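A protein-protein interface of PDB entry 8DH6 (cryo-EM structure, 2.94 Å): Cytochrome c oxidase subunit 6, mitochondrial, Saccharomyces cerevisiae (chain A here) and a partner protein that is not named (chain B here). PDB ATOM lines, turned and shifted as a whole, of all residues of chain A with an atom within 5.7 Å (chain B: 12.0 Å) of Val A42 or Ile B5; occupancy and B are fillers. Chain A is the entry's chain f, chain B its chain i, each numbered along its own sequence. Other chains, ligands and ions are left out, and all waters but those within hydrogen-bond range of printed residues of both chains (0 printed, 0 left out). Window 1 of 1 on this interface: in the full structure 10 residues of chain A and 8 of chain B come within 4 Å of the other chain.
Val A42 touches just one residue of chain B: Ile B5.
Of chain A, only Leu A41 (3.7 Å), Val A42 (3.4 Å), Val A75 (3.7 Å) and Gln A80 (3.2 Å) come within 4 Å of Ile B5.
No residue of chain B comes within 4 Å of Pro A43.
Ala A44 touches none of the printed residues of chain B.
No residue of chain B comes within 4 Å of Leu A71.
No residue of chain B comes within 4 Å of Lys A74.
Printed residues of chain B within 4 Å of Val A75: Ile B5.
Of chain B, only Ile B5 (3.2 Å) comes within 4 Å of Gln A80.
Printed residues of chain A within 4 Å of Ile B9: Asp A40.
Of the printed residues of chain A, Arg B11 touches Glu A76 (3.5 Å).
Of the printed residues of chain A, Thr B6 touches Asp A40 (2.8 Å) and Leu A41 (3.2 Å).
Of the printed residues of chain B, Phe A9 touches Pro B4.
Of the printed residues of chain B, Glu A76 touches Thr B8 (3.2 Å) and Arg B11 (3.5 Å).
The nearest residue of chain B that does not touch Val A42 is Thr B6 (5.2 Å).
The nearest residue of chain A that does not touch Ile B5 is Tyr A84 (4.4 Å).
The side-chain hydroxyl (OG1) of Thr B6 sits at hydrogen-bond distance from the backbone carbonyl oxygen (O) of Asp A40, at 2.8 Å.
O of Asp A40 sits at hydrogen-bond distance from N of Gly B7 (3.0 Å).
The backbone NH (N) of Val A42 is in hydrogen-bond range of the backbone carbonyl oxygen (O) of Ile B5, 3.4 Å away.
OE2 of Glu A76 sits close to OG1 of Thr B8 (3.4 Å).
The side-chain carboxylate (OE2) of Glu A76 is in salt-bridge range of the guanidinium group (NH1) of Arg B11 (3.5 Å).
O of Pro A43 is in hydrogen-bond range of OH of Tyr A84 (3.0 Å).
Among the printed residues, pairs that only touch across the chains: Gln A80 with Ile B5, Leu A41 with Thr B6, Tyr A84 with Ile B2, Phe A9 with Pro B4, Asp A40 with Ile B9, Leu A41 with Ile B5 and Val A75 with Ile B5.
Of the 14 printed residues of chain A, 8 touch a printed residue of chain B.
Hydrophobic or aromatic side chains of chain A that line the printed part of chain B: Phe A9, Leu A41, Val A42, Val A75 and Tyr A84.
Among the printed residues, 12 pairs touch across the chains.
Among the printed residues, Asp or Glu carboxylates within 4 Å of a Lys or Arg side-chain nitrogen of the other chain: Glu A76 with Arg B11.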
ATOM      1  N   PHE A   9       8.739  -8.335 -25.039  1.00  0.00           N
ATOM      2  CA  PHE A   9       9.132  -7.463 -23.937  1.00  0.00           C
ATOM      3  C   PHE A   9       8.591  -7.973 -22.606  1.00  0.00           C
ATOM      4  O   PHE A   9       9.286  -7.915 -21.586  1.00  0.00           O
ATOM      5  CB  PHE A   9       8.654  -6.036 -24.201  1.00  0.00           C
ATOM      6  CG  PHE A   9       9.398  -4.995 -23.419  1.00  0.00           C
ATOM      7  CD1 PHE A   9      10.712  -4.691 -23.723  1.00  0.00           C
ATOM      8  CD2 PHE A   9       8.782  -4.315 -22.383  1.00  0.00           C
ATOM      9  CE1 PHE A   9      11.399  -3.733 -23.007  1.00  0.00           C
ATOM     10  CE2 PHE A   9       9.465  -3.355 -21.664  1.00  0.00           C
ATOM     11  CZ  PHE A   9      10.774  -3.064 -21.978  1.00  0.00           C
ATOM     12  N   PHE A  37      21.182  -5.402 -19.115  1.00  0.00           N
ATOM     13  CA  PHE A  37      21.396  -4.162 -19.849  1.00  0.00           C
ATOM     14  C   PHE A  37      22.117  -4.366 -21.174  1.00  0.00           C
ATOM     15  O   PHE A  37      22.266  -3.402 -21.929  1.00  0.00           O
ATOM     16  CB  PHE A  37      22.177  -3.172 -18.984  1.00  0.00           C
ATOM     17  CG  PHE A  37      21.302  -2.241 -18.201  1.00  0.00           C
ATOM     18  CD1 PHE A  37      20.885  -1.042 -18.745  1.00  0.00           C
ATOM     19  CD2 PHE A  37      20.886  -2.569 -16.924  1.00  0.00           C
ATOM     20  CE1 PHE A  37      20.075  -0.187 -18.029  1.00  0.00           C
ATOM     21  CE2 PHE A  37      20.075  -1.716 -16.204  1.00  0.00           C
ATOM     22  CZ  PHE A  37      19.670  -0.525 -16.757  1.00  0.00           C
ATOM     23  N   TYR A  39      21.240  -5.621 -24.008  1.00  0.00           N
ATOM     24  CA  TYR A  39      20.200  -5.985 -24.961  1.00  0.00           C
ATOM     25  C   TYR A  39      19.842  -4.757 -25.783  1.00  0.00           C
ATOM     26  O   TYR A  39      20.240  -3.634 -25.465  1.00  0.00           O
ATOM     27  CB  TYR A  39      18.963  -6.545 -24.253  1.00  0.00           C
ATOM     28  CG  TYR A  39      19.016  -8.030 -23.987  1.00  0.00           C
ATOM     29  CD1 TYR A  39      18.898  -8.944 -25.021  1.00  0.00           C
ATOM     30  CD2 TYR A  39      19.178  -8.517 -22.702  1.00  0.00           C
ATOM     31  CE1 TYR A  39      18.943 -10.299 -24.782  1.00  0.00           C
ATOM     32  CE2 TYR A  39      19.224  -9.870 -22.454  1.00  0.00           C
ATOM     33  CZ  TYR A  39      19.107 -10.756 -23.495  1.00  0.00           C
ATOM     34  OH  TYR A  39      19.154 -12.106 -23.242  1.00  0.00           O
ATOM     35  N   ASP A  40      19.076  -4.975 -26.846  1.00  0.00           N
ATOM     36  CA  ASP A  40      18.600  -3.876 -27.684  1.00  0.00           C
ATOM     37  C   ASP A  40      17.284  -3.303 -27.165  1.00  0.00           C
ATOM     38  O   ASP A  40      16.317  -3.125 -27.903  1.00  0.00           O
ATOM     39  CB  ASP A  40      18.477  -4.346 -29.131  1.00  0.00           C
ATOM     40  CG  ASP A  40      17.459  -5.464 -29.311  1.00  0.00           C
ATOM     41  OD1 ASP A  40      16.865  -5.918 -28.309  1.00  0.00           O
ATOM     42  OD2 ASP A  40      17.252  -5.891 -30.465  1.00  0.00           O
ATOM     43  N   LEU A  41      17.262  -2.989 -25.872  1.00  0.00           N
ATOM     44  CA  LEU A  41      16.076  -2.459 -25.216  1.00  0.00           C
ATOM     45  C   LEU A  41      16.458  -1.985 -23.823  1.00  0.00           C
ATOM     46  O   LEU A  41      17.327  -2.577 -23.179  1.00  0.00           O
ATOM     47  CB  LEU A  41      14.963  -3.512 -25.137  1.00  0.00           C
ATOM     48  CG  LEU A  41      15.243  -4.823 -24.399  1.00  0.00           C
ATOM     49  CD1 LEU A  41      14.839  -4.724 -22.941  1.00  0.00           C
ATOM     50  CD2 LEU A  41      14.525  -5.981 -25.068  1.00  0.00           C
ATOM     51  N   VAL A  42      15.811  -0.923 -23.371  1.00  0.00           N
ATOM     52  CA  VAL A  42      15.991  -0.456 -21.994  1.00  0.00           C
ATOM     53  C   VAL A  42      15.033  -1.224 -21.089  1.00  0.00           C
ATOM     54  O   VAL A  42      13.833  -1.301 -21.396  1.00  0.00           O
ATOM     55  CB  VAL A  42      15.756   1.046 -21.900  1.00  0.00           C
ATOM     56  CG1 VAL A  42      16.049   1.541 -20.495  1.00  0.00           C
ATOM     57  CG2 VAL A  42      16.641   1.765 -22.898  1.00  0.00           C
ATOM     58  N   PRO A  43      15.515  -1.809 -19.994  1.00  0.00           N
ATOM     59  CA  PRO A  43      14.639  -2.611 -19.134  1.00  0.00           C
ATOM     60  C   PRO A  43      13.496  -1.792 -18.559  1.00  0.00           C
ATOM     61  O   PRO A  43      13.614  -0.589 -18.320  1.00  0.00           O
ATOM     62  CB  PRO A  43      15.579  -3.097 -18.026  1.00  0.00           C
ATOM     63  CG  PRO A  43      16.939  -3.011 -18.615  1.00  0.00           C
ATOM     64  CD  PRO A  43      16.916  -1.845 -19.544  1.00  0.00           C
ATOM     65  N   ALA A  44      12.373  -2.470 -18.342  1.00  0.00           N
ATOM     66  CA  ALA A  44      11.188  -1.814 -17.819  1.00  0.00           C
ATOM     67  C   ALA A  44      11.426  -1.358 -16.381  1.00  0.00           C
ATOM     68  O   ALA A  44      12.329  -1.857 -15.705  1.00  0.00           O
ATOM     69  CB  ALA A  44       9.991  -2.759 -17.879  1.00  0.00           C
ATOM     70  N   LEU A  71      21.123   3.169 -16.917  1.00  0.00           N
ATOM     71  CA  LEU A  71      19.870   3.554 -17.556  1.00  0.00           C
ATOM     72  C   LEU A  71      20.024   4.869 -18.311  1.00  0.00           C
ATOM     73  O   LEU A  71      19.496   5.021 -19.418  1.00  0.00           O
ATOM     74  CB  LEU A  71      18.761   3.652 -16.509  1.00  0.00           C
ATOM     75  CG  LEU A  71      17.318   3.683 -17.013  1.00  0.00           C
ATOM     76  CD1 LEU A  71      16.407   2.998 -16.016  1.00  0.00           C
ATOM     77  CD2 LEU A  71      16.854   5.105 -17.262  1.00  0.00           C
ATOM     78  N   LYS A  74      21.980   4.264 -21.410  1.00  0.00           N
ATOM     79  CA  LYS A  74      21.306   3.315 -22.288  1.00  0.00           C
ATOM     80  C   LYS A  74      20.120   3.933 -23.014  1.00  0.00           C
ATOM     81  O   LYS A  74      19.861   3.599 -24.175  1.00  0.00           O
ATOM     82  CB  LYS A  74      20.831   2.108 -21.475  1.00  0.00           C
ATOM     83  CG  LYS A  74      20.249   0.976 -22.297  1.00  0.00           C
ATOM     84  CD  LYS A  74      21.314   0.287 -23.120  1.00  0.00           C
ATOM     85  CE  LYS A  74      20.812  -1.039 -23.644  1.00  0.00           C
ATOM     86  NZ  LYS A  74      21.934  -1.972 -23.919  1.00  0.00           N
ATOM     87  N   VAL A  75      19.394   4.826 -22.350  1.00  0.00           N
ATOM     88  CA  VAL A  75      18.173   5.378 -22.917  1.00  0.00           C
ATOM     89  C   VAL A  75      18.520   6.356 -24.038  1.00  0.00           C
ATOM     90  O   VAL A  75      19.614   6.923 -24.093  1.00  0.00           O
ATOM     91  CB  VAL A  75      17.329   6.046 -21.818  1.00  0.00           C
ATOM     92  CG1 VAL A  75      18.036   7.271 -21.268  1.00  0.00           C
ATOM     93  CG2 VAL A  75      15.946   6.376 -22.312  1.00  0.00           C
ATOM     94  N   GLU A  76      17.565   6.551 -24.949  1.00  0.00           N
ATOM     95  CA  GLU A  76      17.769   7.369 -26.139  1.00  0.00           C
ATOM     96  C   GLU A  76      17.839   8.860 -25.834  1.00  0.00           C
ATOM     97  O   GLU A  76      18.861   9.499 -26.107  1.00  0.00           O
ATOM     98  CB  GLU A  76      16.644   7.117 -27.146  1.00  0.00           C
ATOM     99  CG  GLU A  76      16.638   5.725 -27.743  1.00  0.00           C
ATOM    100  CD  GLU A  76      15.498   5.520 -28.716  1.00  0.00           C
ATOM    101  OE1 GLU A  76      14.641   6.422 -28.827  1.00  0.00           O
ATOM    102  OE2 GLU A  76      15.454   4.457 -29.366  1.00  0.00           O
ATOM    103  N   GLN A  80      13.348  10.740 -21.736  1.00  0.00           N
ATOM    104  CA  GLN A  80      12.932   9.416 -21.290  1.00  0.00           C
ATOM    105  C   GLN A  80      13.667   8.998 -20.024  1.00  0.00           C
ATOM    106  O   GLN A  80      13.111   8.271 -19.197  1.00  0.00           O
ATOM    107  CB  GLN A  80      13.154   8.401 -22.407  1.00  0.00           C
ATOM    108  CG  GLN A  80      12.760   8.910 -23.780  1.00  0.00           C
ATOM    109  CD  GLN A  80      12.865   7.845 -24.848  1.00  0.00           C
ATOM    110  OE1 GLN A  80      13.026   6.665 -24.550  1.00  0.00           O
ATOM    111  NE2 GLN A  80      12.773   8.258 -26.105  1.00  0.00           N
ATOM    112  N   TYR A  84      11.896   7.946 -16.601  1.00  0.00           N
ATOM    113  CA  TYR A  84      12.254   6.796 -15.778  1.00  0.00           C
ATOM    114  C   TYR A  84      12.486   7.192 -14.325  1.00  0.00           C
ATOM    115  O   TYR A  84      11.954   6.554 -13.411  1.00  0.00           O
ATOM    116  CB  TYR A  84      13.495   6.104 -16.339  1.00  0.00           C
ATOM    117  CG  TYR A  84      13.199   4.945 -17.261  1.00  0.00           C
ATOM    118  CD1 TYR A  84      12.851   3.704 -16.748  1.00  0.00           C
ATOM    119  CD2 TYR A  84      13.272   5.084 -18.638  1.00  0.00           C
ATOM    120  CE1 TYR A  84      12.582   2.639 -17.576  1.00  0.00           C
ATOM    121  CE2 TYR A  84      13.004   4.020 -19.477  1.00  0.00           C
ATOM    122  CZ  TYR A  84      12.659   2.801 -18.939  1.00  0.00           C
ATOM    123  OH  TYR A  84      12.389   1.734 -19.763  1.00  0.00           O
ATOM    124  N   THR B   1       3.160   5.973 -17.104  1.00  0.00           N
ATOM    125  CA  THR B   1       4.096   4.857 -17.144  1.00  0.00           C
ATOM    126  C   THR B   1       5.155   5.069 -18.220  1.00  0.00           C
ATOM    127  O   THR B   1       5.279   6.159 -18.776  1.00  0.00           O
ATOM    128  CB  THR B   1       3.374   3.525 -17.403  1.00  0.00           C
ATOM    129  OG1 THR B   1       2.795   3.541 -18.713  1.00  0.00           O
ATOM    130  CG2 THR B   1       2.282   3.304 -16.371  1.00  0.00           C
ATOM    131  N   ILE B   2       5.919   4.020 -18.508  1.00  0.00           N
ATOM    132  CA  ILE B   2       6.985   4.070 -19.498  1.00  0.00           C
ATOM    133  C   ILE B   2       6.631   3.122 -20.634  1.00  0.00           C
ATOM    134  O   ILE B   2       6.503   1.910 -20.424  1.00  0.00           O
ATOM    135  CB  ILE B   2       8.341   3.700 -18.880  1.00  0.00           C
ATOM    136  CG1 ILE B   2       8.684   4.657 -17.740  1.00  0.00           C
ATOM    137  CG2 ILE B   2       9.427   3.727 -19.938  1.00  0.00           C
ATOM    138  CD1 ILE B   2       8.802   6.090 -18.174  1.00  0.00           C
ATOM    139  N   ALA B   3       6.476   3.668 -21.835  1.00  0.00           N
ATOM    140  CA  ALA B   3       6.233   2.828 -22.996  1.00  0.00           C
ATOM    141  C   ALA B   3       7.484   2.013 -23.314  1.00  0.00           C
ATOM    142  O   ALA B   3       8.601   2.532 -23.224  1.00  0.00           O
ATOM    143  CB  ALA B   3       5.838   3.675 -24.203  1.00  0.00           C
ATOM    144  N   PRO B   4       7.334   0.739 -23.676  1.00  0.00           N
ATOM    145  CA  PRO B   4       8.512  -0.088 -23.968  1.00  0.00           C
ATOM    146  C   PRO B   4       9.323   0.448 -25.135  1.00  0.00           C
ATOM    147  O   PRO B   4       8.854   0.458 -26.276  1.00  0.00           O
ATOM    148  CB  PRO B   4       7.909  -1.462 -24.292  1.00  0.00           C
ATOM    149  CG  PRO B   4       6.467  -1.207 -24.581  1.00  0.00           C
ATOM    150  CD  PRO B   4       6.080  -0.024 -23.762  1.00  0.00           C
ATOM    151  N   ILE B   5      10.544   0.888 -24.858  1.00  0.00           N
ATOM    152  CA  ILE B   5      11.441   1.424 -25.874  1.00  0.00           C
ATOM    153  C   ILE B   5      12.454   0.340 -26.223  1.00  0.00           C
ATOM    154  O   ILE B   5      13.118  -0.221 -25.344  1.00  0.00           O
ATOM    155  CB  ILE B   5      12.107   2.728 -25.411  1.00  0.00           C
ATOM    156  CG1 ILE B   5      12.967   2.507 -24.168  1.00  0.00           C
ATOM    157  CG2 ILE B   5      11.055   3.794 -25.141  1.00  0.00           C
ATOM    158  CD1 ILE B   5      13.813   3.693 -23.813  1.00  0.00           C
ATOM    159  N   THR B   6      12.546   0.018 -27.510  1.00  0.00           N
ATOM    160  CA  THR B   6      13.350  -1.098 -27.979  1.00  0.00           C
ATOM    161  C   THR B   6      13.634  -0.934 -29.464  1.00  0.00           C
ATOM    162  O   THR B   6      13.002  -0.131 -30.154  1.00  0.00           O
ATOM    163  CB  THR B   6      12.650  -2.439 -27.721  1.00  0.00           C
ATOM    164  OG1 THR B   6      13.537  -3.517 -28.041  1.00  0.00           O
ATOM    165  CG2 THR B   6      11.385  -2.551 -28.557  1.00  0.00           C
ATOM    166  N   GLY B   7      14.598  -1.711 -29.948  1.00  0.00           N
ATOM    167  CA  GLY B   7      14.919  -1.715 -31.363  1.00  0.00           C
ATOM    168  C   GLY B   7      15.692  -0.511 -31.845  1.00  0.00           C
ATOM    169  O   GLY B   7      15.675  -0.214 -33.043  1.00  0.00           O
ATOM    170  N   THR B   8      16.373   0.197 -30.943  1.00  0.00           N
ATOM    171  CA  THR B   8      17.162   1.350 -31.355  1.00  0.00           C
ATOM    172  C   THR B   8      18.374   0.960 -32.192  1.00  0.00           C
ATOM    173  O   THR B   8      18.737   1.698 -33.114  1.00  0.00           O
ATOM    174  CB  THR B   8      17.603   2.156 -30.131  1.00  0.00           C
ATOM    175  OG1 THR B   8      18.416   3.260 -30.550  1.00  0.00           O
ATOM    176  CG2 THR B   8      18.381   1.292 -29.154  1.00  0.00           C
ATOM    177  N   ILE B   9      19.003  -0.179 -31.900  1.00  0.00           N
ATOM    178  CA  ILE B   9      20.213  -0.553 -32.622  1.00  0.00           C
ATOM    179  C   ILE B   9      19.904  -0.949 -34.065  1.00  0.00           C
ATOM    180  O   ILE B   9      20.696  -0.663 -34.965  1.00  0.00           O
ATOM    181  CB  ILE B   9      20.968  -1.662 -31.865  1.00  0.00           C
ATOM    182  CG1 ILE B   9      22.416  -1.746 -32.351  1.00  0.00           C
ATOM    183  CG2 ILE B   9      20.270  -3.010 -32.000  1.00  0.00           C
ATOM    184  CD1 ILE B   9      23.242  -0.544 -31.979  1.00  0.00           C
ATOM    185  N   LYS B  10      18.762  -1.596 -34.318  1.00  0.00           N
ATOM    186  CA  LYS B  10      18.384  -1.925 -35.690  1.00  0.00           C
ATOM    187  C   LYS B  10      18.125  -0.665 -36.509  1.00  0.00           C
ATOM    188  O   LYS B  10      18.551  -0.563 -37.669  1.00  0.00           O
ATOM    189  CB  LYS B  10      17.148  -2.825 -35.683  1.00  0.00           C
ATOM    190  CG  LYS B  10      16.620  -3.185 -37.060  1.00  0.00           C
ATOM    191  CD  LYS B  10      15.440  -4.137 -36.956  1.00  0.00           C
ATOM    192  CE  LYS B  10      14.305  -3.528 -36.152  1.00  0.00           C
ATOM    193  NZ  LYS B  10      13.786  -2.280 -36.781  1.00  0.00           N
ATOM    194  N   ARG B  11      17.424   0.300 -35.914  1.00  0.00           N
ATOM    195  CA  ARG B  11      17.179   1.573 -36.579  1.00  0.00           C
ATOM    196  C   ARG B  11      18.484   2.309 -36.850  1.00  0.00           C
ATOM    197  O   ARG B  11      18.677   2.875 -37.934  1.00  0.00           O
ATOM    198  CB  ARG B  11      16.239   2.410 -35.715  1.00  0.00           C
ATOM    199  CG  ARG B  11      16.253   3.895 -35.971  1.00  0.00           C
ATOM    200  CD  ARG B  11      15.425   4.595 -34.910  1.00  0.00           C
ATOM    201  NE  ARG B  11      14.137   3.938 -34.718  1.00  0.00           N
ATOM    202  CZ  ARG B  11      13.758   3.337 -33.598  1.00  0.00           C
ATOM    203  NH1 ARG B  11      14.543   3.299 -32.535  1.00  0.00           N
ATOM    204  NH2 ARG B  11      12.564   2.757 -33.546  1.00  0.00           N
ATOM    205  N   ARG B  12      19.404   2.294 -35.884  1.00  0.00           N
ATOM    206  CA  ARG B  12      20.714   2.893 -36.103  1.00  0.00           C
ATOM    207  C   ARG B  12      21.472   2.191 -37.221  1.00  0.00           C
ATOM    208  O   ARG B  12      22.139   2.851 -38.025  1.00  0.00           O
ATOM    209  CB  ARG B  12      21.524   2.856 -34.809  1.00  0.00           C
ATOM    210  CG  ARG B  12      22.685   3.824 -34.776  1.00  0.00           C
ATOM    211  CD  ARG B  12      23.366   3.815 -33.419  1.00  0.00           C
ATOM    212  NE  ARG B  12      22.501   4.338 -32.368  1.00  0.00           N
ATOM    213  CZ  ARG B  12      22.757   4.240 -31.071  1.00  0.00           C
ATOM    214  NH1 ARG B  12      23.852   3.647 -30.626  1.00  0.00           N
ATOM    215  NH2 ARG B  12      21.895   4.752 -30.199  1.00  0.00           N
